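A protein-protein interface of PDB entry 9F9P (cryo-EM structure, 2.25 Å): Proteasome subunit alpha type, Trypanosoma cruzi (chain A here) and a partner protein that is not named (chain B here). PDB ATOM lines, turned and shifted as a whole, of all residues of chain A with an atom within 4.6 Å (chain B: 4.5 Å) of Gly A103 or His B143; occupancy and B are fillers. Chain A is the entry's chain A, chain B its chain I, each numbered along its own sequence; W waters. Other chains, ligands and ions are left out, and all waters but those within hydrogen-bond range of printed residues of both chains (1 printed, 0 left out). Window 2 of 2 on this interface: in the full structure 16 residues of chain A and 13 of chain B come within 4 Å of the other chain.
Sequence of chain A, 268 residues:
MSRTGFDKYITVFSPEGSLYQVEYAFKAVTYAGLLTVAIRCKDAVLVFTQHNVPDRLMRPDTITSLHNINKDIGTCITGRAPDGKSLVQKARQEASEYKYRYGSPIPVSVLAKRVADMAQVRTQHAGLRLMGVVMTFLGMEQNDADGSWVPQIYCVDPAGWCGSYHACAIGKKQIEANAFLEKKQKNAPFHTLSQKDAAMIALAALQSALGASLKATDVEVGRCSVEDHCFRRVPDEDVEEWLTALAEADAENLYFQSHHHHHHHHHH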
ATOM      1  N   TYR A  98      25.146  -7.673   2.483  1.00  0.00           N
ATOM      2  CA  TYR A  98      24.791  -6.740   3.523  1.00  0.00           C
ATOM      3  C   TYR A  98      25.937  -6.578   4.531  1.00  0.00           C
ATOM      4  O   TYR A  98      26.262  -5.479   4.916  1.00  0.00           O
ATOM      5  CB  TYR A  98      23.463  -7.175   4.167  1.00  0.00           C
ATOM      6  CG  TYR A  98      22.936  -6.272   5.242  1.00  0.00           C
ATOM      7  CD1 TYR A  98      21.853  -5.430   5.019  1.00  0.00           C
ATOM      8  CD2 TYR A  98      23.455  -6.328   6.526  1.00  0.00           C
ATOM      9  CE1 TYR A  98      21.329  -4.618   6.028  1.00  0.00           C
ATOM     10  CE2 TYR A  98      22.959  -5.514   7.551  1.00  0.00           C
ATOM     11  CZ  TYR A  98      21.923  -4.626   7.286  1.00  0.00           C
ATOM     12  OH  TYR A  98      21.476  -3.841   8.344  1.00  0.00           O
ATOM     13  N   LYS A  99      26.576  -7.669   4.916  1.00  0.00           N
ATOM     14  CA  LYS A  99      27.621  -7.695   5.918  1.00  0.00           C
ATOM     15  C   LYS A  99      28.872  -6.984   5.424  1.00  0.00           C
ATOM     16  O   LYS A  99      29.497  -6.262   6.192  1.00  0.00           O
ATOM     17  CB  LYS A  99      27.950  -9.153   6.209  1.00  0.00           C
ATOM     18  CG  LYS A  99      29.102  -9.398   7.152  1.00  0.00           C
ATOM     19  CD  LYS A  99      28.707  -9.821   8.506  1.00  0.00           C
ATOM     20  CE  LYS A  99      29.924 -10.077   9.372  1.00  0.00           C
ATOM     21  NZ  LYS A  99      29.667 -11.227  10.274  1.00  0.00           N
ATOM     22  N   TYR A 100      29.205  -7.151   4.145  1.00  0.00           N
ATOM     23  CA  TYR A 100      30.310  -6.433   3.561  1.00  0.00           C
ATOM     24  C   TYR A 100      30.054  -4.918   3.590  1.00  0.00           C
ATOM     25  O   TYR A 100      30.956  -4.154   3.925  1.00  0.00           O
ATOM     26  CB  TYR A 100      30.625  -6.945   2.141  1.00  0.00           C
ATOM     27  CG  TYR A 100      31.893  -6.376   1.548  1.00  0.00           C
ATOM     28  CD1 TYR A 100      33.154  -6.677   2.078  1.00  0.00           C
ATOM     29  CD2 TYR A 100      31.836  -5.472   0.503  1.00  0.00           C
ATOM     30  CE1 TYR A 100      34.322  -6.107   1.570  1.00  0.00           C
ATOM     31  CE2 TYR A 100      32.984  -4.879  -0.015  1.00  0.00           C
ATOM     32  CZ  TYR A 100      34.229  -5.199   0.517  1.00  0.00           C
ATOM     33  OH  TYR A 100      35.317  -4.564  -0.058  1.00  0.00           O
ATOM     34  N   ARG A 101      28.877  -4.474   3.159  1.00  0.00           N
ATOM     35  CA  ARG A 101      28.538  -3.074   3.020  1.00  0.00           C
ATOM     36  C   ARG A 101      28.389  -2.363   4.387  1.00  0.00           C
ATOM     37  O   ARG A 101      28.878  -1.262   4.550  1.00  0.00           O
ATOM     38  CB  ARG A 101      27.257  -2.978   2.179  1.00  0.00           C
ATOM     39  CG  ARG A 101      26.735  -1.572   1.938  1.00  0.00           C
ATOM     40  CD  ARG A 101      25.541  -1.439   0.996  1.00  0.00           C
ATOM     41  NE  ARG A 101      25.689  -2.210  -0.248  1.00  0.00           N
ATOM     42  CZ  ARG A 101      25.035  -3.342  -0.562  1.00  0.00           C
ATOM     43  NH1 ARG A 101      24.035  -3.795   0.185  1.00  0.00           N
ATOM     44  NH2 ARG A 101      25.396  -4.034  -1.635  1.00  0.00           N
ATOM     45  N   TYR A 102      27.718  -2.954   5.374  1.00  0.00           N
ATOM     46  CA  TYR A 102      27.379  -2.252   6.596  1.00  0.00           C
ATOM     47  C   TYR A 102      28.161  -2.778   7.796  1.00  0.00           C
ATOM     48  O   TYR A 102      28.077  -2.228   8.892  1.00  0.00           O
ATOM     49  CB  TYR A 102      25.892  -2.393   6.907  1.00  0.00           C
ATOM     50  CG  TYR A 102      24.978  -1.805   5.866  1.00  0.00           C
ATOM     51  CD1 TYR A 102      24.908  -0.435   5.668  1.00  0.00           C
ATOM     52  CD2 TYR A 102      24.198  -2.610   5.048  1.00  0.00           C
ATOM     53  CE1 TYR A 102      24.078   0.119   4.706  1.00  0.00           C
ATOM     54  CE2 TYR A 102      23.382  -2.082   4.060  1.00  0.00           C
ATOM     55  CZ  TYR A 102      23.320  -0.709   3.882  1.00  0.00           C
ATOM     56  OH  TYR A 102      22.473  -0.161   2.945  1.00  0.00           O
ATOM     57  N   GLY A 103      28.835  -3.904   7.618  1.00  0.00           N
ATOM     58  CA  GLY A 103      29.750  -4.414   8.615  1.00  0.00           C
ATOM     59  C   GLY A 103      29.093  -5.140   9.774  1.00  0.00           C
ATOM     60  O   GLY A 103      29.769  -5.424  10.751  1.00  0.00           O
ATOM     61  N   SER A 104      27.803  -5.455   9.673  1.00  0.00           N
ATOM     62  CA  SER A 104      27.094  -6.193  10.714  1.00  0.00           C
ATOM     63  C   SER A 104      26.202  -7.243  10.051  1.00  0.00           C
ATOM     64  O   SER A 104      25.781  -7.046   8.919  1.00  0.00           O
ATOM     65  CB  SER A 104      26.256  -5.221  11.532  1.00  0.00           C
ATOM     66  OG  SER A 104      25.946  -5.740  12.815  1.00  0.00           O
ATOM     67  N   ARG B 141      23.689   2.542  13.821  1.00  0.00           N
ATOM     68  CA  ARG B 141      24.783   2.054  14.638  1.00  0.00           C
ATOM     69  C   ARG B 141      26.070   2.762  14.211  1.00  0.00           C
ATOM     70  O   ARG B 141      26.302   2.981  13.016  1.00  0.00           O
ATOM     71  CB  ARG B 141      25.031   0.551  14.442  1.00  0.00           C
ATOM     72  CG  ARG B 141      23.870  -0.409  14.692  1.00  0.00           C
ATOM     73  CD  ARG B 141      23.482  -0.452  16.155  1.00  0.00           C
ATOM     74  NE  ARG B 141      22.461  -1.463  16.458  1.00  0.00           N
ATOM     75  CZ  ARG B 141      22.666  -2.656  17.032  1.00  0.00           C
ATOM     76  NH1 ARG B 141      21.635  -3.437  17.298  1.00  0.00           N
ATOM     77  NH2 ARG B 141      23.878  -3.076  17.351  1.00  0.00           N
ATOM     78  N   VAL B 142      26.932   3.071  15.184  1.00  0.00           N
ATOM     79  CA  VAL B 142      28.140   3.817  14.889  1.00  0.00           C
ATOM     80  C   VAL B 142      29.107   2.952  14.092  1.00  0.00           C
ATOM     81  O   VAL B 142      29.828   3.471  13.261  1.00  0.00           O
ATOM     82  CB  VAL B 142      28.820   4.369  16.162  1.00  0.00           C
ATOM     83  CG1 VAL B 142      29.932   5.337  15.832  1.00  0.00           C
ATOM     84  CG2 VAL B 142      27.903   5.085  17.112  1.00  0.00           C
ATOM     85  N   HIS B 143      29.143   1.642  14.341  1.00  0.00           N
ATOM     86  CA  HIS B 143      29.970   0.758  13.530  1.00  0.00           C
ATOM     87  C   HIS B 143      29.566   0.740  12.049  1.00  0.00           C
ATOM     88  O   HIS B 143      30.410   0.486  11.194  1.00  0.00           O
ATOM     89  CB  HIS B 143      30.106  -0.644  14.156  1.00  0.00           C
ATOM     90  CG  HIS B 143      31.171  -1.504  13.523  1.00  0.00           C
ATOM     91  ND1 HIS B 143      30.917  -2.513  12.601  1.00  0.00           N
ATOM     92  CD2 HIS B 143      32.542  -1.474  13.651  1.00  0.00           C
ATOM     93  CE1 HIS B 143      32.069  -3.073  12.189  1.00  0.00           C
ATOM     94  NE2 HIS B 143      33.069  -2.458  12.822  1.00  0.00           N
ATOM     95  N   GLU B 144      28.296   0.982  11.709  1.00  0.00           N
ATOM     96  CA  GLU B 144      27.875   0.992  10.307  1.00  0.00           C
ATOM     97  C   GLU B 144      28.428   2.217   9.602  1.00  0.00           C
ATOM     98  O   GLU B 144      28.884   2.139   8.484  1.00  0.00           O
ATOM     99  CB  GLU B 144      26.344   0.968  10.102  1.00  0.00           C
ATOM    100  CG  GLU B 144      25.651  -0.272  10.710  1.00  0.00           C
ATOM    101  CD  GLU B 144      24.096  -0.343  10.758  1.00  0.00           C
ATOM    102  OE1 GLU B 144      23.406   0.663  11.191  1.00  0.00           O
ATOM    103  OE2 GLU B 144      23.542  -1.441  10.385  1.00  0.00           O
ATOM    104  N   ALA B 145      28.283   3.371  10.236  1.00  0.00           N
ATOM    105  CA  ALA B 145      28.852   4.600   9.716  1.00  0.00           C
ATOM    106  C   ALA B 145      30.342   4.433   9.438  1.00  0.00           C
ATOM    107  O   ALA B 145      30.820   4.759   8.367  1.00  0.00           O
ATOM    108  CB  ALA B 145      28.625   5.718  10.702  1.00  0.00           C
ATOM    109  N   LEU B 146      31.032   3.882  10.421  1.00  0.00           N
ATOM    110  CA  LEU B 146      32.453   3.626  10.332  1.00  0.00           C
ATOM    111  C   LEU B 146      32.813   2.729   9.163  1.00  0.00           C
ATOM    112  O   LEU B 146      33.732   3.037   8.447  1.00  0.00           O
ATOM    113  CB  LEU B 146      32.970   3.013  11.633  1.00  0.00           C
ATOM    114  CG  LEU B 146      34.480   2.787  11.586  1.00  0.00           C
ATOM    115  CD1 LEU B 146      35.216   4.135  11.590  1.00  0.00           C
ATOM    116  CD2 LEU B 146      34.980   1.876  12.699  1.00  0.00           C
ATOM    117  N   THR B 147      32.054   1.675   8.933  1.00  0.00           N
ATOM    118  CA  THR B 147      32.321   0.792   7.816  1.00  0.00           C
ATOM    119  C   THR B 147      32.085   1.469   6.471  1.00  0.00           C
ATOM    120  O   THR B 147      32.872   1.321   5.547  1.00  0.00           O
ATOM    121  CB  THR B 147      31.487  -0.483   7.936  1.00  0.00           C
ATOM    122  OG1 THR B 147      31.986  -1.213   9.045  1.00  0.00           O
ATOM    123  CG2 THR B 147      31.581  -1.372   6.724  1.00  0.00           C
ATOM    124  N   PHE B 175      30.873   4.931  21.420  1.00  0.00           N
ATOM    125  CA  PHE B 175      31.803   4.474  20.436  1.00  0.00           C
ATOM    126  C   PHE B 175      32.582   5.655  19.879  1.00  0.00           C
ATOM    127  O   PHE B 175      31.987   6.605  19.441  1.00  0.00           O
ATOM    128  CB  PHE B 175      30.998   3.791  19.339  1.00  0.00           C
ATOM    129  CG  PHE B 175      31.767   3.008  18.309  1.00  0.00           C
ATOM    130  CD1 PHE B 175      32.502   3.647  17.331  1.00  0.00           C
ATOM    131  CD2 PHE B 175      31.722   1.632  18.298  1.00  0.00           C
ATOM    132  CE1 PHE B 175      33.232   2.930  16.396  1.00  0.00           C
ATOM    133  CE2 PHE B 175      32.469   0.909  17.385  1.00  0.00           C
ATOM    134  CZ  PHE B 175      33.242   1.553  16.440  1.00  0.00           C
HETATM  135  O   HOH W   1      28.255  -2.613  11.970  1.00  0.00           O
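Of the 8 printed residues of chain B, 3 touch a printed residue of chain A.
Hydrophobic or aromatic side chains of chain B within 4 Å of the printed part of chain A: His B143.
Of the 7 printed residues of chain A, 5 touch a printed residue of chain B.
Hydrophobic or aromatic side chains of chain A within 4 Å of the printed part of chain B: Tyr A98.
Along chain A the printed residues that touch a printed residue of chain B span positions 98 to 103.
Among the printed residues, 7 pairs touch across the chains.
Among the printed residues, merely in contact across the chains: Arg A101 with Thr B147, Tyr A102 with Glu B144, Gly A103 with His B143, Tyr A98 with Glu B144, Gly A103 with Thr B147, Tyr A102 with Thr B147 and Tyr A100 with Thr B147.
Water W1 lies within hydrogen-bond range of a ring nitrogen (ND1) of His B143 (2.7 Å), the backbone carbonyl oxygen (O) of Tyr A102 (3.1 Å) and the backbone carbonyl oxygen (O) of Gly A103 (3.4 Å).
The side-chain carboxylate (OE1) of Glu B144 lies within hydrogen-bond range of the backbone NH (N) of Arg B141 (3.2 Å).
The backbone carbonyl oxygen of His B143 lies within hydrogen-bond range of the side-chain hydroxyl of Thr B147, at 3.2 Å.
Of the printed residues of chain B, Tyr A98 touches Glu B144 (3.8 Å).
Of the printed residues of chain B, Tyr A100 touches Thr B147.
Of the printed residues of chain B, Tyr A102 touches Glu B144 and Thr B147.
Of chain B, only His B143 (3.6 Å) and Thr B147 (3.8 Å) come within 4 Å of Gly A103.
His B143 touches just one residue of chain A: Gly A103 (3.6 Å).
Leu B146 touches none of the printed residues of chain A.
The nearest residue of chain A that does not touch His B143 is Tyr A102 (4.3 Å).
The nearest printed residue of chain B that does not touch Tyr A98 is Thr B147 (7.0 Å).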
